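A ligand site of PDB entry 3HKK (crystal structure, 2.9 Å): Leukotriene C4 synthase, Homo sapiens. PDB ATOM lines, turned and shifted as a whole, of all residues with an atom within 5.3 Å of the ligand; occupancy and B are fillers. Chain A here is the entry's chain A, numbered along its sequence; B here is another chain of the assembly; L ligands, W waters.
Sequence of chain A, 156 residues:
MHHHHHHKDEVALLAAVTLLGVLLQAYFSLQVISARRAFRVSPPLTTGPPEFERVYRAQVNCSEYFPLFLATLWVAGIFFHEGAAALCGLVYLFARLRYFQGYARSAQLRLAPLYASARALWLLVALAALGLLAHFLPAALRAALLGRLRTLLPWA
ND2 of Asn 61 lies within hydrogen-bond range of O8 of the ligand, 2.8 Å away. OH of Tyr 99 lies within hydrogen-bond range of O4 of the ligand (3.0 Å). O1 of the ligand lies within salt-bridge range of NH2 of Arg 36 of chain B, at 2.8 Å. N1 of the ligand lies within hydrogen-bond range of OE1 of Gln 59 of chain B. The guanidinium group (NH1) of Arg 57 is in salt-bridge range of an oxygen (O8) of the ligand. The side-chain carboxylate of Glu 64 is in salt-bridge range of a nitrogen (N1) of the ligand. O6 of the ligand lies within salt-bridge range of NH1 of Arg 110 (2.6 Å). OH of Tyr 103 sits at hydrogen-bond distance from O9 of the ligand, at 2.7 Å. The side-chain hydroxyl of Tyr 65 is in hydrogen-bond range of an oxygen (O3) of the ligand, 2.9 Å away.
The side-chain carboxylate of Glu 64 sits at hydrogen-bond distance from the side-chain amide nitrogen of Gln 59 of chain B (3.0 Å). NH2 of Arg 57 is in hydrogen-bond range of OH of Tyr 56 of chain B (3.0 Å). O of Pro 44 of chain B lies within hydrogen-bond range of NH1 of Arg 36 of chain B (3.3 Å). The side-chain hydroxyl (OH) of Tyr 99 is in hydrogen-bond range of the side-chain amide oxygen (OD1) of Asn 61, at 3.2 Å. The side-chain hydroxyl of Tyr 65 sits at hydrogen-bond distance from the side-chain hydroxyl of Ser 29 of chain B (3.3 Å).
Water W1 lies within hydrogen-bond range of OE1 of Glu 64, NH2 of Arg 57, N1 of the ligand and OH of Tyr 56 of chain B.
Residues that only touch the ligand: Leu 114 (3.4 Å), Ser 29 of chain B (3.7 Å), Val 32 of chain B (3.8 Å), Ile 33 of chain B (3.4 Å), Pro 43 of chain B (3.3 Å) and Tyr 56 of chain B (3.6 Å). Hydrophobic or aromatic side chains within 4 Å of the ligand: Tyr 65, Tyr 99, Tyr 103, Leu 114, Val 32 of chain B, Ile 33 of chain B, Pro 43 of chain B and Tyr 56 of chain B. The nearest printed residue that does not touch the ligand is Leu 111 (4.1 Å).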
ATOM      1  N   ARG A  57      17.086  31.801  25.789  1.00  0.00           N
ATOM      2  CA  ARG A  57      17.814  30.939  24.879  1.00  0.00           C
ATOM      3  C   ARG A  57      17.038  29.694  24.611  1.00  0.00           C
ATOM      4  O   ARG A  57      17.100  29.169  23.497  1.00  0.00           O
ATOM      5  CB  ARG A  57      19.186  30.605  25.432  1.00  0.00           C
ATOM      6  CG  ARG A  57      20.159  31.705  25.239  1.00  0.00           C
ATOM      7  CD  ARG A  57      21.075  31.332  24.108  1.00  0.00           C
ATOM      8  NE  ARG A  57      20.708  31.964  22.852  1.00  0.00           N
ATOM      9  CZ  ARG A  57      20.486  31.314  21.699  1.00  0.00           C
ATOM     10  NH1 ARG A  57      20.579  29.988  21.633  1.00  0.00           N
ATOM     11  NH2 ARG A  57      20.176  32.015  20.623  1.00  0.00           N
ATOM     12  N   ALA A  58      16.319  29.216  25.628  1.00  0.00           N
ATOM     13  CA  ALA A  58      15.424  28.068  25.497  1.00  0.00           C
ATOM     14  C   ALA A  58      14.354  28.323  24.413  1.00  0.00           C
ATOM     15  O   ALA A  58      14.097  27.464  23.557  1.00  0.00           O
ATOM     16  CB  ALA A  58      14.760  27.724  26.843  1.00  0.00           C
ATOM     17  N   ASN A  61      16.121  28.542  20.894  1.00  0.00           N
ATOM     18  CA  ASN A  61      16.587  27.239  20.413  1.00  0.00           C
ATOM     19  C   ASN A  61      15.399  26.430  19.874  1.00  0.00           C
ATOM     20  O   ASN A  61      15.469  25.821  18.803  1.00  0.00           O
ATOM     21  CB  ASN A  61      17.330  26.515  21.546  1.00  0.00           C
ATOM     22  CG  ASN A  61      18.005  25.220  21.090  1.00  0.00           C
ATOM     23  OD1 ASN A  61      17.361  24.157  21.050  1.00  0.00           O
ATOM     24  ND2 ASN A  61      19.283  25.291  20.750  1.00  0.00           N
ATOM     25  N   GLU A  64      14.231  27.774  16.561  1.00  0.00           N
ATOM     26  CA  GLU A  64      15.051  27.551  15.389  1.00  0.00           C
ATOM     27  C   GLU A  64      14.885  26.140  14.852  1.00  0.00           C
ATOM     28  O   GLU A  64      15.181  25.855  13.692  1.00  0.00           O
ATOM     29  CB  GLU A  64      16.513  28.031  15.559  1.00  0.00           C
ATOM     30  CG  GLU A  64      17.531  27.102  16.234  1.00  0.00           C
ATOM     31  CD  GLU A  64      18.773  27.894  16.724  1.00  0.00           C
ATOM     32  OE1 GLU A  64      19.115  28.941  16.097  1.00  0.00           O
ATOM     33  OE2 GLU A  64      19.383  27.496  17.765  1.00  0.00           O
ATOM     34  N   TYR A  65      14.305  25.270  15.694  1.00  0.00           N
ATOM     35  CA  TYR A  65      13.922  23.931  15.285  1.00  0.00           C
ATOM     36  C   TYR A  65      12.455  23.740  14.866  1.00  0.00           C
ATOM     37  O   TYR A  65      12.189  22.656  14.341  1.00  0.00           O
ATOM     38  CB  TYR A  65      14.271  22.949  16.450  1.00  0.00           C
ATOM     39  CG  TYR A  65      15.719  22.678  16.615  1.00  0.00           C
ATOM     40  CD1 TYR A  65      16.329  21.651  15.896  1.00  0.00           C
ATOM     41  CD2 TYR A  65      16.495  23.457  17.477  1.00  0.00           C
ATOM     42  CE1 TYR A  65      17.702  21.401  16.007  1.00  0.00           C
ATOM     43  CE2 TYR A  65      17.871  23.235  17.611  1.00  0.00           C
ATOM     44  CZ  TYR A  65      18.464  22.196  16.861  1.00  0.00           C
ATOM     45  OH  TYR A  65      19.840  21.952  17.002  1.00  0.00           O
ATOM     46  N   TYR A  99      12.262  20.148  27.971  1.00  0.00           N
ATOM     47  CA  TYR A  99      13.482  20.886  27.654  1.00  0.00           C
ATOM     48  C   TYR A  99      13.472  22.418  27.984  1.00  0.00           C
ATOM     49  O   TYR A  99      14.479  23.032  28.496  1.00  0.00           O
ATOM     50  CB  TYR A  99      13.822  20.814  26.142  1.00  0.00           C
ATOM     51  CG  TYR A  99      14.901  21.758  25.615  1.00  0.00           C
ATOM     52  CD1 TYR A  99      16.234  21.338  25.543  1.00  0.00           C
ATOM     53  CD2 TYR A  99      14.594  23.077  25.199  1.00  0.00           C
ATOM     54  CE1 TYR A  99      17.265  22.184  25.075  1.00  0.00           C
ATOM     55  CE2 TYR A  99      15.592  23.949  24.727  1.00  0.00           C
ATOM     56  CZ  TYR A  99      16.937  23.496  24.680  1.00  0.00           C
ATOM     57  OH  TYR A  99      17.956  24.331  24.236  1.00  0.00           O
ATOM     58  N   TYR A 103      16.002  23.888  31.061  1.00  0.00           N
ATOM     59  CA  TYR A 103      16.964  24.948  30.751  1.00  0.00           C
ATOM     60  C   TYR A 103      16.679  26.202  31.576  1.00  0.00           C
ATOM     61  O   TYR A 103      17.599  26.915  31.959  1.00  0.00           O
ATOM     62  CB  TYR A 103      16.834  25.274  29.263  1.00  0.00           C
ATOM     63  CG  TYR A 103      17.999  25.974  28.593  1.00  0.00           C
ATOM     64  CD1 TYR A 103      19.028  26.570  29.322  1.00  0.00           C
ATOM     65  CD2 TYR A 103      18.055  26.052  27.200  1.00  0.00           C
ATOM     66  CE1 TYR A 103      20.090  27.218  28.696  1.00  0.00           C
ATOM     67  CE2 TYR A 103      19.116  26.705  26.550  1.00  0.00           C
ATOM     68  CZ  TYR A 103      20.146  27.295  27.303  1.00  0.00           C
ATOM     69  OH  TYR A 103      21.197  27.935  26.666  1.00  0.00           O
ATOM     70  N   ARG A 110      18.900  21.052  30.584  1.00  0.00           N
ATOM     71  CA  ARG A 110      18.489  21.057  29.185  1.00  0.00           C
ATOM     72  C   ARG A 110      18.884  19.789  28.419  1.00  0.00           C
ATOM     73  O   ARG A 110      18.197  19.391  27.475  1.00  0.00           O
ATOM     74  CB  ARG A 110      19.057  22.270  28.484  1.00  0.00           C
ATOM     75  CG  ARG A 110      20.400  22.022  27.809  1.00  0.00           C
ATOM     76  CD  ARG A 110      21.018  23.320  27.292  1.00  0.00           C
ATOM     77  NE  ARG A 110      22.327  23.073  26.686  1.00  0.00           N
ATOM     78  CZ  ARG A 110      23.460  22.814  27.372  1.00  0.00           C
ATOM     79  NH1 ARG A 110      24.588  22.586  26.725  1.00  0.00           N
ATOM     80  NH2 ARG A 110      23.462  22.770  28.699  1.00  0.00           N
ATOM     81  N   LEU A 111      19.966  19.147  28.837  1.00  0.00           N
ATOM     82  CA  LEU A 111      20.575  18.070  28.061  1.00  0.00           C
ATOM     83  C   LEU A 111      19.786  16.772  27.907  1.00  0.00           C
ATOM     84  O   LEU A 111      19.711  16.205  26.815  1.00  0.00           O
ATOM     85  CB  LEU A 111      21.970  17.798  28.584  1.00  0.00           C
ATOM     86  CG  LEU A 111      22.951  18.957  28.370  1.00  0.00           C
ATOM     87  CD1 LEU A 111      24.214  18.652  29.119  1.00  0.00           C
ATOM     88  CD2 LEU A 111      23.235  19.177  26.902  1.00  0.00           C
ATOM     89  N   LEU A 114      16.850  17.385  25.617  1.00  0.00           N
ATOM     90  CA  LEU A 114      17.368  17.691  24.291  1.00  0.00           C
ATOM     91  C   LEU A 114      17.614  16.399  23.505  1.00  0.00           C
ATOM     92  O   LEU A 114      17.209  16.308  22.348  1.00  0.00           O
ATOM     93  CB  LEU A 114      18.651  18.526  24.307  1.00  0.00           C
ATOM     94  CG  LEU A 114      19.206  18.860  22.901  1.00  0.00           C
ATOM     95  CD1 LEU A 114      18.324  19.845  22.090  1.00  0.00           C
ATOM     96  CD2 LEU A 114      20.655  19.333  22.899  1.00  0.00           C
ATOM     97  N   SER B  29      23.666  22.678  12.738  1.00  0.00           N
ATOM     98  CA  SER B  29      23.454  22.606  14.165  1.00  0.00           C
ATOM     99  C   SER B  29      24.549  21.827  14.853  1.00  0.00           C
ATOM    100  O   SER B  29      25.107  22.296  15.865  1.00  0.00           O
ATOM    101  CB  SER B  29      22.093  22.032  14.492  1.00  0.00           C
ATOM    102  OG  SER B  29      21.144  23.017  14.220  1.00  0.00           O
ATOM    103  N   VAL B  32      27.698  23.903  15.103  1.00  0.00           N
ATOM    104  CA  VAL B  32      27.654  24.844  16.219  1.00  0.00           C
ATOM    105  C   VAL B  32      27.889  24.114  17.551  1.00  0.00           C
ATOM    106  O   VAL B  32      28.538  24.673  18.429  1.00  0.00           O
ATOM    107  CB  VAL B  32      26.338  25.685  16.268  1.00  0.00           C
ATOM    108  CG1 VAL B  32      26.302  26.575  17.502  1.00  0.00           C
ATOM    109  CG2 VAL B  32      26.239  26.540  15.046  1.00  0.00           C
ATOM    110  N   ILE B  33      27.390  22.897  17.703  1.00  0.00           N
ATOM    111  CA  ILE B  33      27.606  22.150  18.940  1.00  0.00           C
ATOM    112  C   ILE B  33      29.104  21.882  19.124  1.00  0.00           C
ATOM    113  O   ILE B  33      29.651  22.040  20.239  1.00  0.00           O
ATOM    114  CB  ILE B  33      26.797  20.823  18.978  1.00  0.00           C
ATOM    115  CG1 ILE B  33      25.299  21.114  19.121  1.00  0.00           C
ATOM    116  CG2 ILE B  33      27.256  19.949  20.145  1.00  0.00           C
ATOM    117  CD1 ILE B  33      24.364  19.909  18.841  1.00  0.00           C
ATOM    118  N   ARG B  36      31.213  24.818  20.140  1.00  0.00           N
ATOM    119  CA  ARG B  36      31.036  25.140  21.558  1.00  0.00           C
ATOM    120  C   ARG B  36      32.084  24.368  22.396  1.00  0.00           C
ATOM    121  O   ARG B  36      32.693  24.930  23.298  1.00  0.00           O
ATOM    122  CB  ARG B  36      29.599  24.822  22.014  1.00  0.00           C
ATOM    123  CG  ARG B  36      28.591  25.917  21.745  1.00  0.00           C
ATOM    124  CD  ARG B  36      27.327  25.755  22.608  1.00  0.00           C
ATOM    125  NE  ARG B  36      26.240  26.672  22.261  1.00  0.00           N
ATOM    126  CZ  ARG B  36      26.084  27.924  22.732  1.00  0.00           C
ATOM    127  NH1 ARG B  36      26.955  28.446  23.578  1.00  0.00           N
ATOM    128  NH2 ARG B  36      25.052  28.666  22.351  1.00  0.00           N
ATOM    129  N   PRO B  43      26.487  27.381  26.959  1.00  0.00           N
ATOM    130  CA  PRO B  43      25.186  27.989  27.228  1.00  0.00           C
ATOM    131  C   PRO B  43      25.093  28.522  28.648  1.00  0.00           C
ATOM    132  O   PRO B  43      25.691  27.958  29.563  1.00  0.00           O
ATOM    133  CB  PRO B  43      24.211  26.817  27.036  1.00  0.00           C
ATOM    134  CG  PRO B  43      24.899  25.926  26.076  1.00  0.00           C
ATOM    135  CD  PRO B  43      26.373  26.034  26.376  1.00  0.00           C
ATOM    136  N   PRO B  44      24.337  29.609  28.829  1.00  0.00           N
ATOM    137  CA  PRO B  44      23.843  30.395  27.699  1.00  0.00           C
ATOM    138  C   PRO B  44      24.969  30.837  26.771  1.00  0.00           C
ATOM    139  O   PRO B  44      25.676  29.990  26.210  1.00  0.00           O
ATOM    140  CB  PRO B  44      23.212  31.616  28.374  1.00  0.00           C
ATOM    141  CG  PRO B  44      22.805  31.122  29.716  1.00  0.00           C
ATOM    142  CD  PRO B  44      23.836  30.111  30.120  1.00  0.00           C
ATOM    143  N   THR B  46      26.313  33.295  23.665  1.00  0.00           N
ATOM    144  CA  THR B  46      26.404  33.073  22.248  1.00  0.00           C
ATOM    145  C   THR B  46      27.543  33.939  21.718  1.00  0.00           C
ATOM    146  O   THR B  46      27.735  34.038  20.515  1.00  0.00           O
ATOM    147  CB  THR B  46      25.042  33.316  21.558  1.00  0.00           C
ATOM    148  OG1 THR B  46      24.536  34.592  21.954  1.00  0.00           O
ATOM    149  CG2 THR B  46      24.030  32.290  21.987  1.00  0.00           C
ATOM    150  N   TYR B  56      28.386  30.197  14.806  1.00  0.00           N
ATOM    151  CA  TYR B  56      27.093  30.542  15.379  1.00  0.00           C
ATOM    152  C   TYR B  56      26.214  31.399  14.443  1.00  0.00           C
ATOM    153  O   TYR B  56      25.025  31.152  14.269  1.00  0.00           O
ATOM    154  CB  TYR B  56      27.282  31.278  16.701  1.00  0.00           C
ATOM    155  CG  TYR B  56      25.993  31.765  17.297  1.00  0.00           C
ATOM    156  CD1 TYR B  56      25.099  30.866  17.897  1.00  0.00           C
ATOM    157  CD2 TYR B  56      25.661  33.110  17.257  1.00  0.00           C
ATOM    158  CE1 TYR B  56      23.901  31.303  18.431  1.00  0.00           C
ATOM    159  CE2 TYR B  56      24.466  33.556  17.789  1.00  0.00           C
ATOM    160  CZ  TYR B  56      23.589  32.655  18.371  1.00  0.00           C
ATOM    161  OH  TYR B  56      22.392  33.109  18.888  1.00  0.00           O
ATOM    162  N   GLN B  59      24.969  29.643  11.191  1.00  0.00           N
ATOM    163  CA  GLN B  59      23.853  28.745  11.446  1.00  0.00           C
ATOM    164  C   GLN B  59      22.565  29.532  11.683  1.00  0.00           C
ATOM    165  O   GLN B  59      21.485  29.118  11.223  1.00  0.00           O
ATOM    166  CB  GLN B  59      24.162  27.789  12.593  1.00  0.00           C
ATOM    167  CG  GLN B  59      23.006  26.915  13.027  1.00  0.00           C
ATOM    168  CD  GLN B  59      22.242  27.515  14.210  1.00  0.00           C
ATOM    169  OE1 GLN B  59      22.800  27.726  15.286  1.00  0.00           O
ATOM    170  NE2 GLN B  59      20.959  27.799  14.006  1.00  0.00           N
ATOM    171  N   VAL B  60      22.656  30.657  12.376  1.00  0.00           N
ATOM    172  CA  VAL B  60      21.485  31.412  12.701  1.00  0.00           C
ATOM    173  C   VAL B  60      20.931  32.075  11.432  1.00  0.00           C
ATOM    174  O   VAL B  60      19.720  32.084  11.192  1.00  0.00           O
ATOM    175  CB  VAL B  60      21.788  32.458  13.810  1.00  0.00           C
ATOM    176  CG1 VAL B  60      20.632  33.419  13.996  1.00  0.00           C
ATOM    177  CG2 VAL B  60      22.128  31.753  15.130  1.00  0.00           C
HETATM  178  N1  LIG L   1      21.893  27.668  18.007  1.00  0.00           N
HETATM  179  C1  LIG L   1      22.229  26.504  18.826  1.00  0.00           C
HETATM  180  C2  LIG L   1      23.264  26.895  19.902  1.00  0.00           C
HETATM  181  O1  LIG L   1      23.748  28.071  19.947  1.00  0.00           O
HETATM  182  O2  LIG L   1      23.601  26.032  20.772  1.00  0.00           O
HETATM  183  C3  LIG L   1      22.559  25.345  17.844  1.00  0.00           C
HETATM  184  C4  LIG L   1      23.032  24.014  18.425  1.00  0.00           C
HETATM  185  C5  LIG L   1      22.153  23.505  19.543  1.00  0.00           C
HETATM  186  O3  LIG L   1      20.957  23.357  19.343  1.00  0.00           O
HETATM  187  N2  LIG L   1      22.772  23.264  20.712  1.00  0.00           N
HETATM  188  C6  LIG L   1      22.151  22.695  21.900  1.00  0.00           C
HETATM  189  C7  LIG L   1      21.665  23.707  22.907  1.00  0.00           C
HETATM  190  O4  LIG L   1      20.823  23.421  23.776  1.00  0.00           O
HETATM  191  C8  LIG L   1      23.072  21.663  22.573  1.00  0.00           C
HETATM  192  S1  LIG L   1      24.559  22.191  23.163  1.00  0.00           S
HETATM  193  O5  LIG L   1      25.482  22.752  22.143  1.00  0.00           O
HETATM  194  O6  LIG L   1      24.346  23.241  24.207  1.00  0.00           O
HETATM  195  O7  LIG L   1      25.191  20.997  23.734  1.00  0.00           O
HETATM  196  N3  LIG L   1      22.184  24.929  22.767  1.00  0.00           N
HETATM  197  C9  LIG L   1      21.945  25.973  23.744  1.00  0.00           C
HETATM  198  C10 LIG L   1      21.253  27.201  23.192  1.00  0.00           C
HETATM  199  O8  LIG L   1      20.814  27.200  22.006  1.00  0.00           O
HETATM  200  O9  LIG L   1      21.138  28.185  23.964  1.00  0.00           O
HETATM  201  O   HOH W   1      20.330  30.453  18.135  1.00  0.00           O
